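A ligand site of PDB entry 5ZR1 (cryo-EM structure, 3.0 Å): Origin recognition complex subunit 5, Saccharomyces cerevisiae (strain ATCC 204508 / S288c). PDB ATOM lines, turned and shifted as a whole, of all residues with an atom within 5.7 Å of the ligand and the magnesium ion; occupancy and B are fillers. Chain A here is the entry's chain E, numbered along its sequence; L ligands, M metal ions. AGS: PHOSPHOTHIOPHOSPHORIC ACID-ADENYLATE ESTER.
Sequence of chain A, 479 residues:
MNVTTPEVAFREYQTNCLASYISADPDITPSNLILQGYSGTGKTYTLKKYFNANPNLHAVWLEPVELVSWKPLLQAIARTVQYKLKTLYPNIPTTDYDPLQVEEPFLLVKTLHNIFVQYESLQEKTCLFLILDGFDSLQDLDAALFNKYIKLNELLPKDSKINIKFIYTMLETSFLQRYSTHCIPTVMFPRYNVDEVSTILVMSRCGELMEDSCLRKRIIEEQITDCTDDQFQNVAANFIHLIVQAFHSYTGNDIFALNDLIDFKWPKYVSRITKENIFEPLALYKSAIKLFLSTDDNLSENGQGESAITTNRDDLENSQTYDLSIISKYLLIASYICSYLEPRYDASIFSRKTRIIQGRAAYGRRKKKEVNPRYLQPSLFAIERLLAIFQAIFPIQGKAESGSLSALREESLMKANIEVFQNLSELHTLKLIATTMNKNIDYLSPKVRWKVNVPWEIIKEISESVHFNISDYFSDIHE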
ATOM      1  N   VAL A   8      15.860 -16.466 -16.278  1.00  0.00           N
ATOM      2  CA  VAL A   8      16.728 -15.344 -15.964  1.00  0.00           C
ATOM      3  C   VAL A   8      16.023 -14.540 -14.878  1.00  0.00           C
ATOM      4  O   VAL A   8      14.784 -14.497 -14.843  1.00  0.00           O
ATOM      5  CB  VAL A   8      17.028 -14.519 -17.237  1.00  0.00           C
ATOM      6  CG1 VAL A   8      18.045 -13.422 -16.987  1.00  0.00           C
ATOM      7  CG2 VAL A   8      17.518 -15.427 -18.344  1.00  0.00           C
ATOM      8  N   ALA A   9      16.802 -13.924 -13.981  1.00  0.00           N
ATOM      9  CA  ALA A   9      16.294 -13.511 -12.684  1.00  0.00           C
ATOM     10  C   ALA A   9      15.282 -12.370 -12.782  1.00  0.00           C
ATOM     11  O   ALA A   9      14.120 -12.517 -12.402  1.00  0.00           O
ATOM     12  CB  ALA A   9      17.466 -13.105 -11.779  1.00  0.00           C
ATOM     13  N   PHE A  10      15.715 -11.222 -13.283  1.00  0.00           N
ATOM     14  CA  PHE A  10      14.853 -10.042 -13.338  1.00  0.00           C
ATOM     15  C   PHE A  10      14.511  -9.663 -14.774  1.00  0.00           C
ATOM     16  O   PHE A  10      14.226  -8.497 -15.072  1.00  0.00           O
ATOM     17  CB  PHE A  10      15.521  -8.882 -12.609  1.00  0.00           C
ATOM     18  CG  PHE A  10      15.684  -9.126 -11.138  1.00  0.00           C
ATOM     19  CD1 PHE A  10      14.620  -8.956 -10.274  1.00  0.00           C
ATOM     20  CD2 PHE A  10      16.898  -9.550 -10.631  1.00  0.00           C
ATOM     21  CE1 PHE A  10      14.767  -9.190  -8.920  1.00  0.00           C
ATOM     22  CE2 PHE A  10      17.051  -9.792  -9.277  1.00  0.00           C
ATOM     23  CZ  PHE A  10      15.983  -9.601  -8.431  1.00  0.00           C
ATOM     24  N   ARG A  11      14.505 -10.648 -15.671  1.00  0.00           N
ATOM     25  CA  ARG A  11      14.252 -10.449 -17.080  1.00  0.00           C
ATOM     26  C   ARG A  11      13.159 -11.400 -17.563  1.00  0.00           C
ATOM     27  O   ARG A  11      13.244 -11.915 -18.680  1.00  0.00           O
ATOM     28  CB  ARG A  11      15.511 -10.705 -17.904  1.00  0.00           C
ATOM     29  CG  ARG A  11      16.744  -9.917 -17.514  1.00  0.00           C
ATOM     30  CD  ARG A  11      16.834  -8.503 -18.053  1.00  0.00           C
ATOM     31  NE  ARG A  11      16.169  -7.502 -17.225  1.00  0.00           N
ATOM     32  CZ  ARG A  11      16.185  -6.200 -17.500  1.00  0.00           C
ATOM     33  NH1 ARG A  11      15.561  -5.353 -16.704  1.00  0.00           N
ATOM     34  NH2 ARG A  11      16.862  -5.756 -18.535  1.00  0.00           N
ATOM     35  N   GLY A  37      18.828  -2.144 -24.993  1.00  0.00           N
ATOM     36  CA  GLY A  37      18.913  -1.666 -23.629  1.00  0.00           C
ATOM     37  C   GLY A  37      20.204  -0.906 -23.479  1.00  0.00           C
ATOM     38  O   GLY A  37      21.093  -0.987 -24.331  1.00  0.00           O
ATOM     39  N   TYR A  38      20.338  -0.179 -22.379  1.00  0.00           N
ATOM     40  CA  TYR A  38      21.581   0.530 -22.117  1.00  0.00           C
ATOM     41  C   TYR A  38      22.623  -0.435 -21.556  1.00  0.00           C
ATOM     42  O   TYR A  38      22.438  -1.652 -21.536  1.00  0.00           O
ATOM     43  CB  TYR A  38      21.323   1.725 -21.216  1.00  0.00           C
ATOM     44  CG  TYR A  38      20.824   2.892 -22.024  1.00  0.00           C
ATOM     45  CD1 TYR A  38      21.730   3.748 -22.626  1.00  0.00           C
ATOM     46  CD2 TYR A  38      19.474   3.093 -22.244  1.00  0.00           C
ATOM     47  CE1 TYR A  38      21.302   4.807 -23.386  1.00  0.00           C
ATOM     48  CE2 TYR A  38      19.038   4.147 -23.008  1.00  0.00           C
ATOM     49  CZ  TYR A  38      19.958   4.990 -23.575  1.00  0.00           C
ATOM     50  OH  TYR A  38      19.541   6.056 -24.339  1.00  0.00           O
ATOM     51  N   SER A  39      23.753   0.109 -21.128  1.00  0.00           N
ATOM     52  CA  SER A  39      24.880  -0.721 -20.719  1.00  0.00           C
ATOM     53  C   SER A  39      24.605  -1.396 -19.386  1.00  0.00           C
ATOM     54  O   SER A  39      23.992  -0.813 -18.496  1.00  0.00           O
ATOM     55  CB  SER A  39      26.151   0.119 -20.625  1.00  0.00           C
ATOM     56  OG  SER A  39      27.230  -0.670 -20.182  1.00  0.00           O
ATOM     57  N   GLY A  40      25.047  -2.645 -19.276  1.00  0.00           N
ATOM     58  CA  GLY A  40      24.890  -3.401 -18.046  1.00  0.00           C
ATOM     59  C   GLY A  40      23.491  -3.872 -17.742  1.00  0.00           C
ATOM     60  O   GLY A  40      23.252  -4.352 -16.634  1.00  0.00           O
ATOM     61  N   THR A  41      22.566  -3.761 -18.685  1.00  0.00           N
ATOM     62  CA  THR A  41      21.170  -4.112 -18.450  1.00  0.00           C
ATOM     63  C   THR A  41      20.867  -5.570 -18.724  1.00  0.00           C
ATOM     64  O   THR A  41      19.681  -5.936 -18.771  1.00  0.00           O
ATOM     65  CB  THR A  41      20.246  -3.234 -19.285  1.00  0.00           C
ATOM     66  OG1 THR A  41      20.597  -3.382 -20.662  1.00  0.00           O
ATOM     67  CG2 THR A  41      20.379  -1.788 -18.876  1.00  0.00           C
ATOM     68  N   GLY A  42      21.882  -6.407 -18.895  1.00  0.00           N
ATOM     69  CA  GLY A  42      21.682  -7.838 -18.948  1.00  0.00           C
ATOM     70  C   GLY A  42      21.002  -8.330 -20.207  1.00  0.00           C
ATOM     71  O   GLY A  42      20.051  -9.100 -20.131  1.00  0.00           O
ATOM     72  N   LYS A  43      21.489  -7.893 -21.362  1.00  0.00           N
ATOM     73  CA  LYS A  43      20.875  -8.282 -22.622  1.00  0.00           C
ATOM     74  C   LYS A  43      21.754  -9.168 -23.484  1.00  0.00           C
ATOM     75  O   LYS A  43      21.247  -9.741 -24.452  1.00  0.00           O
ATOM     76  CB  LYS A  43      20.446  -7.058 -23.429  1.00  0.00           C
ATOM     77  CG  LYS A  43      21.557  -6.158 -23.863  1.00  0.00           C
ATOM     78  CD  LYS A  43      21.012  -4.922 -24.516  1.00  0.00           C
ATOM     79  CE  LYS A  43      22.123  -3.984 -24.861  1.00  0.00           C
ATOM     80  NZ  LYS A  43      22.755  -3.417 -23.648  1.00  0.00           N
ATOM     81  N   THR A  44      23.048  -9.285 -23.177  1.00  0.00           N
ATOM     82  CA  THR A  44      23.823 -10.395 -23.692  1.00  0.00           C
ATOM     83  C   THR A  44      23.856 -11.561 -22.720  1.00  0.00           C
ATOM     84  O   THR A  44      24.242 -12.658 -23.101  1.00  0.00           O
ATOM     85  CB  THR A  44      25.264  -9.981 -23.981  1.00  0.00           C
ATOM     86  OG1 THR A  44      25.924  -9.647 -22.760  1.00  0.00           O
ATOM     87  CG2 THR A  44      25.273  -8.773 -24.868  1.00  0.00           C
ATOM     88  N   TYR A  45      23.464 -11.325 -21.462  1.00  0.00           N
ATOM     89  CA  TYR A  45      23.316 -12.418 -20.517  1.00  0.00           C
ATOM     90  C   TYR A  45      22.143 -13.299 -20.904  1.00  0.00           C
ATOM     91  O   TYR A  45      22.300 -14.505 -21.145  1.00  0.00           O
ATOM     92  CB  TYR A  45      23.133 -11.874 -19.098  1.00  0.00           C
ATOM     93  CG  TYR A  45      23.049 -12.946 -18.040  1.00  0.00           C
ATOM     94  CD1 TYR A  45      24.189 -13.575 -17.563  1.00  0.00           C
ATOM     95  CD2 TYR A  45      21.819 -13.336 -17.506  1.00  0.00           C
ATOM     96  CE1 TYR A  45      24.120 -14.545 -16.596  1.00  0.00           C
ATOM     97  CE2 TYR A  45      21.743 -14.310 -16.543  1.00  0.00           C
ATOM     98  CZ  TYR A  45      22.891 -14.911 -16.089  1.00  0.00           C
ATOM     99  OH  TYR A  45      22.815 -15.886 -15.126  1.00  0.00           O
ATOM    100  N   ASP A 133      25.896  -8.276 -32.105  1.00  0.00           N
ATOM    101  CA  ASP A 133      25.779  -7.998 -30.681  1.00  0.00           C
ATOM    102  C   ASP A 133      26.494  -6.690 -30.364  1.00  0.00           C
ATOM    103  O   ASP A 133      27.687  -6.669 -30.066  1.00  0.00           O
ATOM    104  CB  ASP A 133      26.354  -9.152 -29.880  1.00  0.00           C
ATOM    105  CG  ASP A 133      26.081  -9.035 -28.421  1.00  0.00           C
ATOM    106  OD1 ASP A 133      24.921  -9.276 -28.030  1.00  0.00           O
ATOM    107  OD2 ASP A 133      27.015  -8.680 -27.668  1.00  0.00           O
ATOM    108  N   THR A 169      21.560  -5.927 -31.297  1.00  0.00           N
ATOM    109  CA  THR A 169      21.698  -5.474 -29.928  1.00  0.00           C
ATOM    110  C   THR A 169      22.220  -4.051 -29.993  1.00  0.00           C
ATOM    111  O   THR A 169      23.206  -3.801 -30.683  1.00  0.00           O
ATOM    112  CB  THR A 169      22.628  -6.409 -29.150  1.00  0.00           C
ATOM    113  OG1 THR A 169      22.011  -7.687 -28.978  1.00  0.00           O
ATOM    114  CG2 THR A 169      22.990  -5.848 -27.823  1.00  0.00           C
ATOM    115  N   LEU A 171      22.120   0.213 -28.028  1.00  0.00           N
ATOM    116  CA  LEU A 171      22.148   0.878 -26.732  1.00  0.00           C
ATOM    117  C   LEU A 171      21.216   2.089 -26.619  1.00  0.00           C
ATOM    118  O   LEU A 171      20.352   2.115 -25.748  1.00  0.00           O
ATOM    119  CB  LEU A 171      23.586   1.320 -26.430  1.00  0.00           C
ATOM    120  CG  LEU A 171      24.613   0.258 -26.024  1.00  0.00           C
ATOM    121  CD1 LEU A 171      26.004   0.787 -26.204  1.00  0.00           C
ATOM    122  CD2 LEU A 171      24.422  -0.097 -24.582  1.00  0.00           C
ATOM    123  N   TYR A 192      18.130  -1.559 -14.240  1.00  0.00           N
ATOM    124  CA  TYR A 192      17.725  -2.287 -13.056  1.00  0.00           C
ATOM    125  C   TYR A 192      17.426  -1.337 -11.910  1.00  0.00           C
ATOM    126  O   TYR A 192      17.769  -0.149 -11.935  1.00  0.00           O
ATOM    127  CB  TYR A 192      18.788  -3.290 -12.641  1.00  0.00           C
ATOM    128  CG  TYR A 192      18.980  -4.446 -13.585  1.00  0.00           C
ATOM    129  CD1 TYR A 192      18.017  -5.433 -13.693  1.00  0.00           C
ATOM    130  CD2 TYR A 192      20.146  -4.594 -14.331  1.00  0.00           C
ATOM    131  CE1 TYR A 192      18.167  -6.494 -14.540  1.00  0.00           C
ATOM    132  CE2 TYR A 192      20.314  -5.667 -15.174  1.00  0.00           C
ATOM    133  CZ  TYR A 192      19.327  -6.609 -15.269  1.00  0.00           C
ATOM    134  OH  TYR A 192      19.456  -7.696 -16.099  1.00  0.00           O
ATOM    135  N   ILE A 200      21.496  -9.199  -8.211  1.00  0.00           N
ATOM    136  CA  ILE A 200      22.335  -9.700  -9.294  1.00  0.00           C
ATOM    137  C   ILE A 200      23.799  -9.703  -8.882  1.00  0.00           C
ATOM    138  O   ILE A 200      24.531 -10.668  -9.155  1.00  0.00           O
ATOM    139  CB  ILE A 200      22.085  -8.851 -10.557  1.00  0.00           C
ATOM    140  CG1 ILE A 200      20.743  -9.228 -11.171  1.00  0.00           C
ATOM    141  CG2 ILE A 200      23.217  -8.957 -11.555  1.00  0.00           C
ATOM    142  CD1 ILE A 200      20.291  -8.277 -12.216  1.00  0.00           C
ATOM    143  N   MET A 203      24.582 -12.675  -6.402  1.00  0.00           N
ATOM    144  CA  MET A 203      24.631 -14.020  -6.974  1.00  0.00           C
ATOM    145  C   MET A 203      25.740 -14.166  -8.004  1.00  0.00           C
ATOM    146  O   MET A 203      26.113 -15.293  -8.331  1.00  0.00           O
ATOM    147  CB  MET A 203      23.293 -14.396  -7.619  1.00  0.00           C
ATOM    148  CG  MET A 203      22.941 -13.612  -8.865  1.00  0.00           C
ATOM    149  SD  MET A 203      21.414 -14.162  -9.650  1.00  0.00           S
ATOM    150  CE  MET A 203      20.193 -13.549  -8.505  1.00  0.00           C
ATOM    151  N   SER A 204      26.265 -13.052  -8.507  1.00  0.00           N
ATOM    152  CA  SER A 204      27.359 -13.086  -9.458  1.00  0.00           C
ATOM    153  C   SER A 204      28.724 -13.122  -8.784  1.00  0.00           C
ATOM    154  O   SER A 204      29.660 -13.699  -9.349  1.00  0.00           O
ATOM    155  CB  SER A 204      27.300 -11.864 -10.383  1.00  0.00           C
ATOM    156  OG  SER A 204      28.388 -11.840 -11.277  1.00  0.00           O
ATOM    157  N   ILE A 255      26.316  -2.092 -13.244  1.00  0.00           N
ATOM    158  CA  ILE A 255      26.869  -3.353 -12.774  1.00  0.00           C
ATOM    159  C   ILE A 255      28.395  -3.329 -12.799  1.00  0.00           C
ATOM    160  O   ILE A 255      29.027  -3.882 -11.887  1.00  0.00           O
ATOM    161  CB  ILE A 255      26.317  -4.524 -13.613  1.00  0.00           C
ATOM    162  CG1 ILE A 255      24.791  -4.525 -13.592  1.00  0.00           C
ATOM    163  CG2 ILE A 255      26.804  -5.874 -13.093  1.00  0.00           C
ATOM    164  CD1 ILE A 255      24.190  -4.755 -12.232  1.00  0.00           C
ATOM    165  N   PHE A 256      28.989  -2.651 -13.777  1.00  0.00           N
ATOM    166  CA  PHE A 256      30.422  -2.693 -13.996  1.00  0.00           C
ATOM    167  C   PHE A 256      31.178  -1.721 -13.096  1.00  0.00           C
ATOM    168  O   PHE A 256      32.367  -1.931 -12.825  1.00  0.00           O
ATOM    169  CB  PHE A 256      30.707  -2.409 -15.471  1.00  0.00           C
ATOM    170  CG  PHE A 256      30.166  -3.456 -16.396  1.00  0.00           C
ATOM    171  CD1 PHE A 256      30.064  -4.774 -15.984  1.00  0.00           C
ATOM    172  CD2 PHE A 256      29.689  -3.111 -17.642  1.00  0.00           C
ATOM    173  CE1 PHE A 256      29.544  -5.733 -16.821  1.00  0.00           C
ATOM    174  CE2 PHE A 256      29.164  -4.062 -18.480  1.00  0.00           C
ATOM    175  CZ  PHE A 256      29.095  -5.383 -18.075  1.00  0.00           C
ATOM    176  N   ASN A 259      31.120  -3.675  -9.782  1.00  0.00           N
ATOM    177  CA  ASN A 259      32.101  -4.758  -9.851  1.00  0.00           C
ATOM    178  C   ASN A 259      33.534  -4.265  -9.730  1.00  0.00           C
ATOM    179  O   ASN A 259      34.402  -5.049  -9.345  1.00  0.00           O
ATOM    180  CB  ASN A 259      31.950  -5.528 -11.162  1.00  0.00           C
ATOM    181  CG  ASN A 259      30.839  -6.545 -11.107  1.00  0.00           C
ATOM    182  OD1 ASN A 259      30.709  -7.281 -10.141  1.00  0.00           O
ATOM    183  ND2 ASN A 259      30.037  -6.597 -12.161  1.00  0.00           N
HETATM  184  PG  AGS L   1      26.621  -3.893 -22.586  1.00  0.00           P
HETATM  185  S1G AGS L   1      27.982  -2.885 -21.633  1.00  0.00           S
HETATM  186  O2G AGS L   1      26.094  -3.030 -23.765  1.00  0.00           O
HETATM  187  O3G AGS L   1      27.272  -5.181 -23.169  1.00  0.00           O
HETATM  188  PB  AGS L   1      25.032  -5.761 -21.423  1.00  0.00           P
HETATM  189  O1B AGS L   1      23.515  -5.776 -21.290  1.00  0.00           O
HETATM  190  O2B AGS L   1      25.532  -6.543 -22.549  1.00  0.00           O
HETATM  191  O3B AGS L   1      25.437  -4.263 -21.644  1.00  0.00           O
HETATM  192  PA  AGS L   1      26.029  -7.783 -19.794  1.00  0.00           P
HETATM  193  O1A AGS L   1      24.767  -8.635 -19.651  1.00  0.00           O
HETATM  194  O2A AGS L   1      26.986  -8.278 -20.790  1.00  0.00           O
HETATM  195  O3A AGS L   1      25.584  -6.290 -20.033  1.00  0.00           O
HETATM  196  O5' AGS L   1      26.807  -7.715 -18.432  1.00  0.00           O
HETATM  197  C5' AGS L   1      26.130  -7.508 -17.184  1.00  0.00           C
HETATM  198  C4' AGS L   1      26.835  -8.307 -16.122  1.00  0.00           C
HETATM  199  O4' AGS L   1      25.929  -8.589 -15.046  1.00  0.00           O
HETATM  200  C3' AGS L   1      27.339  -9.675 -16.577  1.00  0.00           C
HETATM  201  O3' AGS L   1      28.452 -10.086 -15.808  1.00  0.00           O
HETATM  202  C2' AGS L   1      26.125 -10.576 -16.347  1.00  0.00           C
HETATM  203  O2' AGS L   1      26.530 -11.902 -16.049  1.00  0.00           O
HETATM  204  C1' AGS L   1      25.467  -9.929 -15.124  1.00  0.00           C
HETATM  205  N9  AGS L   1      24.018  -9.906 -15.187  1.00  0.00           N
HETATM  206  C8  AGS L   1      23.245  -9.009 -15.871  1.00  0.00           C
HETATM  207  N7  AGS L   1      21.958  -9.221 -15.766  1.00  0.00           N
HETATM  208  C5  AGS L   1      21.874 -10.337 -14.944  1.00  0.00           C
HETATM  209  C6  AGS L   1      20.784 -11.065 -14.446  1.00  0.00           C
HETATM  210  N6  AGS L   1      19.507 -10.770 -14.711  1.00  0.00           N
HETATM  211  N1  AGS L   1      21.052 -12.132 -13.658  1.00  0.00           N
HETATM  212  C2  AGS L   1      22.322 -12.432 -13.398  1.00  0.00           C
HETATM  213  N3  AGS L   1      23.432 -11.819 -13.804  1.00  0.00           N
HETATM  214  C4  AGS L   1      23.141 -10.767 -14.584  1.00  0.00           C
HETATM  215 MG    MG M   1      26.987  -7.089 -24.124  1.00  0.00          MG
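Val 8 touches the ligand (CG1 to N6, 3.8 Å). Tyr 38 touches the ligand. CD2 of Leu 171 touches O2G of the ligand, at 3.5 Å. Ile 200 touches the ligand (CG2 to C4, 3.5 Å). Ile 255 touches the ligand. Phe 256 touches the ligand. 14 residues have an atom within 4 Å of the ligand: Val 8, Tyr 38, Ser 39, Gly 40, Thr 41, Gly 42, Lys 43, Thr 44, Tyr 45, Leu 171, Tyr 192, Ile 200, Ile 255 and Phe 256. Along chain A the residues within 4 Å of the ligand span positions 8 to 256. The nearest printed residue that does not touch the ligand is Arg 11 (4.03 Å).
The side-chain amino group of Lys 43 lies within hydrogen-bond range of the backbone carbonyl oxygen of Tyr 38, 2.8 Å away. The backbone carbonyl oxygen of Gly 37 sits at hydrogen-bond distance from the side-chain amino group of Lys 43 (3.0 Å). OH of Tyr 192 is in hydrogen-bond range of O of Thr 41. OH of Tyr 192 lies close to NE of Arg 11 (3.5 Å). The backbone carbonyl oxygen (O) of Tyr 38 is in hydrogen-bond range of the side-chain hydroxyl (OG1) of Thr 41 (2.7 Å). The guanidinium group (NH2) of Arg 11 sits at hydrogen-bond distance from the backbone carbonyl oxygen (O) of Thr 41 (2.8 Å). The side-chain amide nitrogen (ND2) of Asn 259 lies within hydrogen-bond range of the backbone carbonyl oxygen (O) of Ile 255 (2.9 Å). OD1 of Asp 133 lies within hydrogen-bond range of OG1 of Thr 169 (3.4 Å).
Residues that only touch the magnesium ion: Thr 44 (2.5 Å) and Asp 133 (3.9 Å). Of the 23 residues printed, 2 come within 4 Å of the magnesium ion.
The magnesium ion is bound by O3G of the ligand (2.2 Å) and O2B of the ligand (2.2 Å).
The side-chain hydroxyl (OG1) of Thr 44 lies within hydrogen-bond range of an oxygen (O2A) of the ligand, 2.6 Å away. OG of Ser 39 sits close to S1G of the ligand, 2.8 Å away. The backbone NH (N) of Gly 40 lies within hydrogen-bond range of an oxygen (O3B) of the ligand (2.9 Å). N of Lys 43 sits at hydrogen-bond distance from O1B of the ligand, 2.9 Å away. NZ of Lys 43 lies within salt-bridge range of O1B of the ligand (3.4 Å). The side-chain hydroxyl (OH) of Tyr 192 sits at hydrogen-bond distance from a nitrogen (N7) of the ligand. The backbone NH (N) of Gly 42 is in hydrogen-bond range of an oxygen (O1B) of the ligand (3.0 Å). N of Tyr 45 is in hydrogen-bond range of O1A of the ligand. An oxygen (O1B) of the ligand sits at hydrogen-bond distance from the backbone NH (N) of Thr 41 (3.4 Å).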
